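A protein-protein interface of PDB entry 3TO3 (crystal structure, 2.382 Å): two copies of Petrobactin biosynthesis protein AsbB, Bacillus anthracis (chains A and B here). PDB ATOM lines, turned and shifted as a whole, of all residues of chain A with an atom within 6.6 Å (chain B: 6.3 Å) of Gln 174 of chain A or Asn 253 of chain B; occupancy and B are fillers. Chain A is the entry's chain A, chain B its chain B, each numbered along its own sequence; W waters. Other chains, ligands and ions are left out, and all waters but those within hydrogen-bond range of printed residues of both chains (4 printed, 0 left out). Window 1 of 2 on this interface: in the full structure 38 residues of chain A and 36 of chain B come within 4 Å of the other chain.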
ATOM      1  N   HIS A 123      12.570  36.181   5.069  1.00  0.00           N
ATOM      2  CA  HIS A 123      12.364  34.914   5.758  1.00  0.00           C
ATOM      3  C   HIS A 123      11.420  33.947   4.995  1.00  0.00           C
ATOM      4  O   HIS A 123      11.673  32.755   4.915  1.00  0.00           O
ATOM      5  CB  HIS A 123      11.821  35.161   7.160  1.00  0.00           C
ATOM      6  CG  HIS A 123      11.664  33.911   7.974  1.00  0.00           C
ATOM      7  ND1 HIS A 123      12.727  33.105   8.315  1.00  0.00           N
ATOM      8  CD2 HIS A 123      10.567  33.333   8.523  1.00  0.00           C
ATOM      9  CE1 HIS A 123      12.297  32.090   9.040  1.00  0.00           C
ATOM     10  NE2 HIS A 123      10.989  32.210   9.183  1.00  0.00           N
ATOM     11  N   GLN A 127      12.343  30.292   3.374  1.00  0.00           N
ATOM     12  CA  GLN A 127      11.544  29.121   3.751  1.00  0.00           C
ATOM     13  C   GLN A 127      10.924  28.427   2.534  1.00  0.00           C
ATOM     14  O   GLN A 127      10.866  27.197   2.483  1.00  0.00           O
ATOM     15  CB  GLN A 127      10.483  29.516   4.796  1.00  0.00           C
ATOM     16  CG  GLN A 127      11.123  29.849   6.140  1.00  0.00           C
ATOM     17  CD  GLN A 127      11.969  28.674   6.610  1.00  0.00           C
ATOM     18  OE1 GLN A 127      11.454  27.556   6.780  1.00  0.00           O
ATOM     19  NE2 GLN A 127      13.273  28.906   6.788  1.00  0.00           N
ATOM     20  N   PHE A 130      13.588  26.478   1.003  1.00  0.00           N
ATOM     21  CA  PHE A 130      13.817  25.337   1.870  1.00  0.00           C
ATOM     22  C   PHE A 130      12.759  24.264   1.649  1.00  0.00           C
ATOM     23  O   PHE A 130      13.090  23.113   1.348  1.00  0.00           O
ATOM     24  CB  PHE A 130      13.802  25.794   3.326  1.00  0.00           C
ATOM     25  CG  PHE A 130      14.042  24.688   4.322  1.00  0.00           C
ATOM     26  CD1 PHE A 130      15.281  24.065   4.415  1.00  0.00           C
ATOM     27  CD2 PHE A 130      13.046  24.298   5.182  1.00  0.00           C
ATOM     28  CE1 PHE A 130      15.515  23.059   5.331  1.00  0.00           C
ATOM     29  CE2 PHE A 130      13.281  23.276   6.124  1.00  0.00           C
ATOM     30  CZ  PHE A 130      14.501  22.660   6.188  1.00  0.00           C
ATOM     31  N   LYS A 131      11.490  24.647   1.767  1.00  0.00           N
ATOM     32  CA  LYS A 131      10.394  23.683   1.654  1.00  0.00           C
ATOM     33  C   LYS A 131      10.191  23.158   0.252  1.00  0.00           C
ATOM     34  O   LYS A 131       9.899  21.975   0.066  1.00  0.00           O
ATOM     35  CB  LYS A 131       9.082  24.267   2.175  1.00  0.00           C
ATOM     36  CG  LYS A 131       8.866  24.018   3.684  1.00  0.00           C
ATOM     37  CD  LYS A 131       8.895  25.332   4.473  1.00  0.00           C
ATOM     38  CE  LYS A 131       9.020  25.064   5.978  1.00  0.00           C
ATOM     39  NZ  LYS A 131       8.884  26.340   6.729  1.00  0.00           N
ATOM     40  N   ARG A 170       5.190  28.246   4.467  1.00  0.00           N
ATOM     41  CA  ARG A 170       4.777  27.381   5.548  1.00  0.00           C
ATOM     42  C   ARG A 170       5.364  27.803   6.900  1.00  0.00           C
ATOM     43  O   ARG A 170       5.990  26.975   7.602  1.00  0.00           O
ATOM     44  CB  ARG A 170       5.105  25.925   5.204  1.00  0.00           C
ATOM     45  CG  ARG A 170       4.068  25.317   4.308  1.00  0.00           C
ATOM     46  CD  ARG A 170       4.586  24.089   3.640  1.00  0.00           C
ATOM     47  NE  ARG A 170       3.701  23.683   2.558  1.00  0.00           N
ATOM     48  CZ  ARG A 170       3.845  22.569   1.849  1.00  0.00           C
ATOM     49  NH1 ARG A 170       4.841  21.732   2.109  1.00  0.00           N
ATOM     50  NH2 ARG A 170       2.981  22.293   0.881  1.00  0.00           N
ATOM     51  N   GLY A 172       5.972  28.414  10.558  1.00  0.00           N
ATOM     52  CA  GLY A 172       5.495  27.576  11.629  1.00  0.00           C
ATOM     53  C   GLY A 172       5.774  26.097  11.433  1.00  0.00           C
ATOM     54  O   GLY A 172       5.737  25.358  12.422  1.00  0.00           O
ATOM     55  N   PHE A 173       6.059  25.657  10.198  1.00  0.00           N
ATOM     56  CA  PHE A 173       6.534  24.283   9.975  1.00  0.00           C
ATOM     57  C   PHE A 173       8.078  24.208   9.973  1.00  0.00           C
ATOM     58  O   PHE A 173       8.746  24.919   9.210  1.00  0.00           O
ATOM     59  CB  PHE A 173       6.013  23.689   8.657  1.00  0.00           C
ATOM     60  CG  PHE A 173       4.644  23.080   8.744  1.00  0.00           C
ATOM     61  CD1 PHE A 173       3.883  23.172   9.912  1.00  0.00           C
ATOM     62  CD2 PHE A 173       4.106  22.408   7.642  1.00  0.00           C
ATOM     63  CE1 PHE A 173       2.607  22.613   9.978  1.00  0.00           C
ATOM     64  CE2 PHE A 173       2.839  21.842   7.699  1.00  0.00           C
ATOM     65  CZ  PHE A 173       2.077  21.943   8.873  1.00  0.00           C
ATOM     66  N   GLN A 174       8.645  23.370  10.843  1.00  0.00           N
ATOM     67  CA  GLN A 174      10.036  22.984  10.681  1.00  0.00           C
ATOM     68  C   GLN A 174      10.020  21.696   9.856  1.00  0.00           C
ATOM     69  O   GLN A 174       8.947  21.253   9.435  1.00  0.00           O
ATOM     70  CB  GLN A 174      10.728  22.838  12.038  1.00  0.00           C
ATOM     71  CG  GLN A 174      10.869  24.192  12.741  1.00  0.00           C
ATOM     72  CD  GLN A 174      11.587  25.230  11.849  1.00  0.00           C
ATOM     73  OE1 GLN A 174      11.097  26.353  11.660  1.00  0.00           O
ATOM     74  NE2 GLN A 174      12.755  24.847  11.297  1.00  0.00           N
ATOM     75  N   TYR A 175      11.178  21.099   9.601  1.00  0.00           N
ATOM     76  CA  TYR A 175      11.225  20.000   8.619  1.00  0.00           C
ATOM     77  C   TYR A 175      10.383  18.706   8.925  1.00  0.00           C
ATOM     78  O   TYR A 175       9.752  18.140   8.019  1.00  0.00           O
ATOM     79  CB  TYR A 175      12.679  19.675   8.234  1.00  0.00           C
ATOM     80  CG  TYR A 175      13.326  18.620   9.088  1.00  0.00           C
ATOM     81  CD1 TYR A 175      13.095  17.272   8.857  1.00  0.00           C
ATOM     82  CD2 TYR A 175      14.237  18.965  10.083  1.00  0.00           C
ATOM     83  CE1 TYR A 175      13.747  16.278   9.624  1.00  0.00           C
ATOM     84  CE2 TYR A 175      14.880  17.983  10.857  1.00  0.00           C
ATOM     85  CZ  TYR A 175      14.625  16.648  10.627  1.00  0.00           C
ATOM     86  OH  TYR A 175      15.258  15.695  11.397  1.00  0.00           O
ATOM     87  N   ARG A 176      10.342  18.261  10.180  1.00  0.00           N
ATOM     88  CA  ARG A 176       9.544  17.076  10.501  1.00  0.00           C
ATOM     89  C   ARG A 176       8.025  17.302  10.325  1.00  0.00           C
ATOM     90  O   ARG A 176       7.372  16.498   9.689  1.00  0.00           O
ATOM     91  CB  ARG A 176       9.890  16.458  11.870  1.00  0.00           C
ATOM     92  CG  ARG A 176      11.385  16.341  12.131  1.00  0.00           C
ATOM     93  CD  ARG A 176      11.667  15.497  13.376  1.00  0.00           C
ATOM     94  NE  ARG A 176      11.349  14.107  13.086  1.00  0.00           N
ATOM     95  CZ  ARG A 176      12.211  13.235  12.562  1.00  0.00           C
ATOM     96  NH1 ARG A 176      13.462  13.599  12.303  1.00  0.00           N
ATOM     97  NH2 ARG A 176      11.822  11.988  12.310  1.00  0.00           N
ATOM     98  N   ASP A 177       7.470  18.386  10.861  1.00  0.00           N
ATOM     99  CA  ASP A 177       6.065  18.682  10.587  1.00  0.00           C
ATOM    100  C   ASP A 177       5.822  18.784   9.071  1.00  0.00           C
ATOM    101  O   ASP A 177       4.828  18.250   8.572  1.00  0.00           O
ATOM    102  CB  ASP A 177       5.599  19.961  11.284  1.00  0.00           C
ATOM    103  CG  ASP A 177       5.252  19.764  12.763  1.00  0.00           C
ATOM    104  OD1 ASP A 177       4.901  18.626  13.209  1.00  0.00           O
ATOM    105  OD2 ASP A 177       5.323  20.789  13.490  1.00  0.00           O
ATOM    106  N   ASN A 178       6.724  19.459   8.345  1.00  0.00           N
ATOM    107  CA  ASN A 178       6.593  19.545   6.896  1.00  0.00           C
ATOM    108  C   ASN A 178       6.496  18.188   6.188  1.00  0.00           C
ATOM    109  O   ASN A 178       5.642  18.011   5.333  1.00  0.00           O
ATOM    110  CB  ASN A 178       7.723  20.368   6.257  1.00  0.00           C
ATOM    111  CG  ASN A 178       7.436  20.694   4.791  1.00  0.00           C
ATOM    112  OD1 ASN A 178       6.498  21.423   4.500  1.00  0.00           O
ATOM    113  ND2 ASN A 178       8.215  20.115   3.868  1.00  0.00           N
ATOM    114  N   PHE A 179       7.389  17.253   6.512  1.00  0.00           N
ATOM    115  CA  PHE A 179       7.282  15.884   5.993  1.00  0.00           C
ATOM    116  C   PHE A 179       5.941  15.185   6.315  1.00  0.00           C
ATOM    117  O   PHE A 179       5.437  14.416   5.500  1.00  0.00           O
ATOM    118  CB  PHE A 179       8.428  15.001   6.531  1.00  0.00           C
ATOM    119  CG  PHE A 179       9.680  15.045   5.706  1.00  0.00           C
ATOM    120  CD1 PHE A 179       9.624  14.951   4.320  1.00  0.00           C
ATOM    121  CD2 PHE A 179      10.924  15.191   6.316  1.00  0.00           C
ATOM    122  CE1 PHE A 179      10.781  14.986   3.566  1.00  0.00           C
ATOM    123  CE2 PHE A 179      12.087  15.221   5.564  1.00  0.00           C
ATOM    124  CZ  PHE A 179      12.026  15.112   4.182  1.00  0.00           C
ATOM    125  N   ASP B 177       8.003  19.115  22.263  1.00  0.00           N
ATOM    126  CA  ASP B 177       9.336  19.638  22.494  1.00  0.00           C
ATOM    127  C   ASP B 177       9.556  19.992  23.963  1.00  0.00           C
ATOM    128  O   ASP B 177      10.657  19.824  24.498  1.00  0.00           O
ATOM    129  CB  ASP B 177       9.598  20.864  21.617  1.00  0.00           C
ATOM    130  CG  ASP B 177       9.975  20.489  20.178  1.00  0.00           C
ATOM    131  OD1 ASP B 177      10.549  19.392  19.948  1.00  0.00           O
ATOM    132  OD2 ASP B 177       9.698  21.312  19.281  1.00  0.00           O
ATOM    133  N   TYR B 181      12.844  18.633  25.853  1.00  0.00           N
ATOM    134  CA  TYR B 181      13.919  19.491  26.318  1.00  0.00           C
ATOM    135  C   TYR B 181      13.748  20.280  27.604  1.00  0.00           C
ATOM    136  O   TYR B 181      14.722  20.868  28.085  1.00  0.00           O
ATOM    137  CB  TYR B 181      14.316  20.423  25.178  1.00  0.00           C
ATOM    138  CG  TYR B 181      14.592  19.624  23.962  1.00  0.00           C
ATOM    139  CD1 TYR B 181      15.671  18.730  23.931  1.00  0.00           C
ATOM    140  CD2 TYR B 181      13.779  19.721  22.849  1.00  0.00           C
ATOM    141  CE1 TYR B 181      15.926  17.945  22.801  1.00  0.00           C
ATOM    142  CE2 TYR B 181      14.030  18.954  21.706  1.00  0.00           C
ATOM    143  CZ  TYR B 181      15.100  18.073  21.686  1.00  0.00           C
ATOM    144  OH  TYR B 181      15.327  17.312  20.566  1.00  0.00           O
ATOM    145  N   PRO B 248      20.337  19.819  19.939  1.00  0.00           N
ATOM    146  CA  PRO B 248      19.577  19.153  18.873  1.00  0.00           C
ATOM    147  C   PRO B 248      18.268  19.867  18.528  1.00  0.00           C
ATOM    148  O   PRO B 248      17.859  19.740  17.376  1.00  0.00           O
ATOM    149  CB  PRO B 248      19.305  17.742  19.436  1.00  0.00           C
ATOM    150  CG  PRO B 248      19.402  17.894  20.937  1.00  0.00           C
ATOM    151  CD  PRO B 248      20.360  19.049  21.198  1.00  0.00           C
ATOM    152  N   TRP B 249      17.642  20.605  19.452  1.00  0.00           N
ATOM    153  CA  TRP B 249      16.430  21.385  19.067  1.00  0.00           C
ATOM    154  C   TRP B 249      16.836  22.517  18.145  1.00  0.00           C
ATOM    155  O   TRP B 249      16.138  22.831  17.178  1.00  0.00           O
ATOM    156  CB  TRP B 249      15.653  22.003  20.252  1.00  0.00           C
ATOM    157  CG  TRP B 249      14.359  22.678  19.854  1.00  0.00           C
ATOM    158  CD1 TRP B 249      13.110  22.123  19.873  1.00  0.00           C
ATOM    159  CD2 TRP B 249      14.187  24.027  19.365  1.00  0.00           C
ATOM    160  NE1 TRP B 249      12.182  23.033  19.444  1.00  0.00           N
ATOM    161  CE2 TRP B 249      12.810  24.206  19.121  1.00  0.00           C
ATOM    162  CE3 TRP B 249      15.063  25.105  19.137  1.00  0.00           C
ATOM    163  CZ2 TRP B 249      12.275  25.410  18.634  1.00  0.00           C
ATOM    164  CZ3 TRP B 249      14.535  26.317  18.665  1.00  0.00           C
ATOM    165  CH2 TRP B 249      13.153  26.450  18.412  1.00  0.00           C
ATOM    166  N   GLN B 250      17.968  23.129  18.457  1.00  0.00           N
ATOM    167  CA  GLN B 250      18.452  24.250  17.676  1.00  0.00           C
ATOM    168  C   GLN B 250      18.814  23.785  16.278  1.00  0.00           C
ATOM    169  O   GLN B 250      18.491  24.453  15.286  1.00  0.00           O
ATOM    170  CB  GLN B 250      19.649  24.905  18.339  1.00  0.00           C
ATOM    171  CG  GLN B 250      20.169  26.077  17.530  1.00  0.00           C
ATOM    172  CD  GLN B 250      19.378  27.336  17.808  1.00  0.00           C
ATOM    173  OE1 GLN B 250      18.247  27.279  18.280  1.00  0.00           O
ATOM    174  NE2 GLN B 250      19.975  28.476  17.547  1.00  0.00           N
ATOM    175  N   TRP B 251      19.434  22.613  16.196  1.00  0.00           N
ATOM    176  CA  TRP B 251      19.888  22.101  14.904  1.00  0.00           C
ATOM    177  C   TRP B 251      18.690  21.803  14.002  1.00  0.00           C
ATOM    178  O   TRP B 251      18.635  22.246  12.866  1.00  0.00           O
ATOM    179  CB  TRP B 251      20.779  20.859  15.065  1.00  0.00           C
ATOM    180  CG  TRP B 251      21.114  20.150  13.792  1.00  0.00           C
ATOM    181  CD1 TRP B 251      20.673  18.925  13.412  1.00  0.00           C
ATOM    182  CD2 TRP B 251      21.965  20.613  12.728  1.00  0.00           C
ATOM    183  NE1 TRP B 251      21.172  18.593  12.188  1.00  0.00           N
ATOM    184  CE2 TRP B 251      21.973  19.607  11.740  1.00  0.00           C
ATOM    185  CE3 TRP B 251      22.708  21.785  12.509  1.00  0.00           C
ATOM    186  CZ2 TRP B 251      22.701  19.729  10.534  1.00  0.00           C
ATOM    187  CZ3 TRP B 251      23.446  21.905  11.320  1.00  0.00           C
ATOM    188  CH2 TRP B 251      23.431  20.875  10.347  1.00  0.00           C
ATOM    189  N   GLU B 252      17.724  21.074  14.522  1.00  0.00           N
ATOM    190  CA  GLU B 252      16.612  20.651  13.688  1.00  0.00           C
ATOM    191  C   GLU B 252      15.550  21.707  13.441  1.00  0.00           C
ATOM    192  O   GLU B 252      14.801  21.599  12.484  1.00  0.00           O
ATOM    193  CB  GLU B 252      15.928  19.447  14.318  1.00  0.00           C
ATOM    194  CG  GLU B 252      16.697  18.173  14.207  1.00  0.00           C
ATOM    195  CD  GLU B 252      15.892  17.008  14.742  1.00  0.00           C
ATOM    196  OE1 GLU B 252      15.889  16.822  15.976  1.00  0.00           O
ATOM    197  OE2 GLU B 252      15.243  16.301  13.936  1.00  0.00           O
ATOM    198  N   ASN B 253      15.337  22.597  14.401  1.00  0.00           N
ATOM    199  CA  ASN B 253      14.293  23.598  14.234  1.00  0.00           C
ATOM    200  C   ASN B 253      14.726  24.961  13.773  1.00  0.00           C
ATOM    201  O   ASN B 253      13.895  25.814  13.459  1.00  0.00           O
ATOM    202  CB  ASN B 253      13.403  23.650  15.462  1.00  0.00           C
ATOM    203  CG  ASN B 253      12.882  22.283  15.812  1.00  0.00           C
ATOM    204  OD1 ASN B 253      12.079  21.719  15.069  1.00  0.00           O
ATOM    205  ND2 ASN B 253      13.374  21.711  16.908  1.00  0.00           N
ATOM    206  N   PHE B 254      16.036  25.170  13.769  1.00  0.00           N
ATOM    207  CA  PHE B 254      16.565  26.476  13.439  1.00  0.00           C
ATOM    208  C   PHE B 254      17.720  26.505  12.425  1.00  0.00           C
ATOM    209  O   PHE B 254      17.632  27.166  11.379  1.00  0.00           O
ATOM    210  CB  PHE B 254      16.792  27.352  14.683  1.00  0.00           C
ATOM    211  CG  PHE B 254      16.910  28.799  14.353  1.00  0.00           C
ATOM    212  CD1 PHE B 254      15.775  29.568  14.163  1.00  0.00           C
ATOM    213  CD2 PHE B 254      18.166  29.388  14.170  1.00  0.00           C
ATOM    214  CE1 PHE B 254      15.874  30.920  13.834  1.00  0.00           C
ATOM    215  CE2 PHE B 254      18.278  30.724  13.836  1.00  0.00           C
ATOM    216  CZ  PHE B 254      17.133  31.499  13.672  1.00  0.00           C
ATOM    217  N   ILE B 255      18.835  25.864  12.778  1.00  0.00           N
ATOM    218  CA  ILE B 255      19.985  25.811  11.884  1.00  0.00           C
ATOM    219  C   ILE B 255      19.658  25.212  10.507  1.00  0.00           C
ATOM    220  O   ILE B 255      19.872  25.857   9.490  1.00  0.00           O
ATOM    221  CB  ILE B 255      21.190  25.050  12.480  1.00  0.00           C
ATOM    222  CG1 ILE B 255      21.454  25.468  13.912  1.00  0.00           C
ATOM    223  CG2 ILE B 255      22.437  25.351  11.653  1.00  0.00           C
ATOM    224  CD1 ILE B 255      21.680  26.941  14.060  1.00  0.00           C
ATOM    225  N   ILE B 256      19.132  23.995  10.477  1.00  0.00           N
ATOM    226  CA  ILE B 256      18.881  23.328   9.208  1.00  0.00           C
ATOM    227  C   ILE B 256      18.012  24.181   8.312  1.00  0.00           C
ATOM    228  O   ILE B 256      18.244  24.261   7.105  1.00  0.00           O
ATOM    229  CB  ILE B 256      18.179  21.973   9.386  1.00  0.00           C
ATOM    230  CG1 ILE B 256      19.116  20.966  10.017  1.00  0.00           C
ATOM    231  CG2 ILE B 256      17.812  21.392   8.051  1.00  0.00           C
ATOM    232  CD1 ILE B 256      18.667  19.544   9.826  1.00  0.00           C
ATOM    233  N   SER B 257      16.980  24.797   8.881  1.00  0.00           N
ATOM    234  CA  SER B 257      16.051  25.522   8.034  1.00  0.00           C
ATOM    235  C   SER B 257      16.546  26.913   7.675  1.00  0.00           C
ATOM    236  O   SER B 257      16.188  27.425   6.624  1.00  0.00           O
ATOM    237  CB  SER B 257      14.663  25.585   8.658  1.00  0.00           C
ATOM    238  OG  SER B 257      14.728  26.207   9.923  1.00  0.00           O
ATOM    239  N   ASN B 258      17.287  27.566   8.570  1.00  0.00           N
ATOM    240  CA  ASN B 258      17.798  28.917   8.267  1.00  0.00           C
ATOM    241  C   ASN B 258      19.217  29.047   7.684  1.00  0.00           C
ATOM    242  O   ASN B 258      19.666  30.130   7.345  1.00  0.00           O
ATOM    243  CB  ASN B 258      17.700  29.793   9.516  1.00  0.00           C
ATOM    244  CG  ASN B 258      16.250  30.053   9.938  1.00  0.00           C
ATOM    245  OD1 ASN B 258      15.698  29.352  10.784  1.00  0.00           O
ATOM    246  ND2 ASN B 258      15.656  31.086   9.376  1.00  0.00           N
HETATM  247  O   HOH W   1      12.379  28.452  10.236  1.00  0.00           O
HETATM  248  O   HOH W   2      13.436  22.281  10.040  1.00  0.00           O
HETATM  249  O   HOH W   3      11.509  19.698  12.843  1.00  0.00           O
HETATM  250  O   HOH W   4      14.932  31.352   6.851  1.00  0.00           O
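The side-chain amino group of Lys 131 of chain A lies within hydrogen-bond range of the side-chain amide oxygen of Gln 127 of chain A (2.8 Å). The backbone carbonyl oxygen of Trp 249 of chain B sits at hydrogen-bond distance from the side-chain amide nitrogen of Asn 253 of chain B. The backbone carbonyl oxygen of Trp 251 of chain B is in hydrogen-bond range of the backbone NH of Ile 256 of chain B. The backbone carbonyl oxygen of Phe 254 of chain B sits at hydrogen-bond distance from the side-chain hydroxyl of Ser 257 of chain B, 3.4 Å away. OD1 of Asn 258 of chain B sits close to O of Phe 254 of chain B (3.0 Å). OG of Ser 257 of chain B lies within hydrogen-bond range of OD1 of Asn 258 of chain B, at 3.4 Å.
Among the printed residues, pairs that only touch across the chains: Phe 130 of chain A with Ile 256 of chain B (3.5 Å), His 123 of chain A with Asn 258 of chain B (3.5 Å) and Phe 130 of chain A with Ser 257 of chain B (3.7 Å).
Of the 13 printed residues of chain A, 6 touch a printed residue of chain B. Printed residues of chain A that touch a printed residue of chain B: His 123, Gln 127, Phe 130, Gln 174, Tyr 175 and Arg 176. Hydrophobic or aromatic side chains of chain A that line the printed part of chain B: His 123, Phe 130 and Tyr 175. Of the 13 printed residues of chain B, 5 touch a printed residue of chain A. Hydrophobic or aromatic side chains of chain B within 4 Å of the printed part of chain A: Ile 256. Among the printed residues, 8 pairs touch across the chains. Among the printed residues, Asp or Glu carboxylates within 4 Å of a Lys or Arg side-chain nitrogen of the other chain: Arg 176 of chain A with Glu 252 of chain B.
Water W2 lies within hydrogen-bond range of N of Tyr 175 of chain A (2.6 Å), O of Glu 252 of chain B (2.9 Å) and NE2 of Gln 174 of chain A (2.9 Å). Water W4 lies within hydrogen-bond range of the side-chain amide nitrogen of Asn 258 of chain B (2.6 Å), the side-chain amide nitrogen of Gln 127 of chain A (3.0 Å) and a ring nitrogen (ND1) of His 123 of chain A (3.2 Å). Water W1 lies within hydrogen-bond range of the side-chain amide oxygen (OE1) of Gln 174 of chain A (2.8 Å), the side-chain hydroxyl (OG) of Ser 257 of chain B (3.3 Å) and the side-chain amide oxygen (OD1) of Asn 258 of chain B (3.5 Å). Water W3 lies within hydrogen-bond range of the side-chain amide oxygen (OD1) of Asn 253 of chain B (3.1 Å) and the backbone NH (N) of Arg 176 of chain A (3.2 Å).
Of the printed residues of chain B, Gln 174 of chain A touches Asn 253 and Ser 257. Asp 177 of chain A touches none of the printed residues of chain B. Asn 253 of chain B touches just one residue of chain A: Gln 174 (2.6 Å). Ile 255 of chain B touches none of the printed residues of chain A. Of the printed residues of chain A, Ser 257 of chain B touches Gln 127, Phe 130 and Gln 174. Printed residues of chain A within 4 Å of Asn 258 of chain B: His 123. The nearest printed residue of chain B that does not touch Gln 174 of chain A is Glu 252 of chain B (4.02 Å). The nearest printed residue of chain B that does not touch Arg 176 of chain A is Asn 253 of chain B (6.2 Å).
1 position is printed for both chains.
The backbone carbonyl oxygen of Ser 257 of chain B is in hydrogen-bond range of the side-chain amide nitrogen of Gln 127 of chain A (3.3 Å). NE2 of Gln 174 of chain A lies within hydrogen-bond range of O of Asn 253 of chain B (2.6 Å). The side-chain hydroxyl (OG) of Ser 257 of chain B is in hydrogen-bond range of the side-chain amide nitrogen (NE2) of Gln 174 of chain A (2.8 Å). OH of Tyr 175 of chain A is in hydrogen-bond range of OE2 of Glu 252 of chain B (2.6 Å). OE2 of Glu 252 of chain B lies within salt-bridge range of NH1 of Arg 176 of chain A (3.6 Å).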
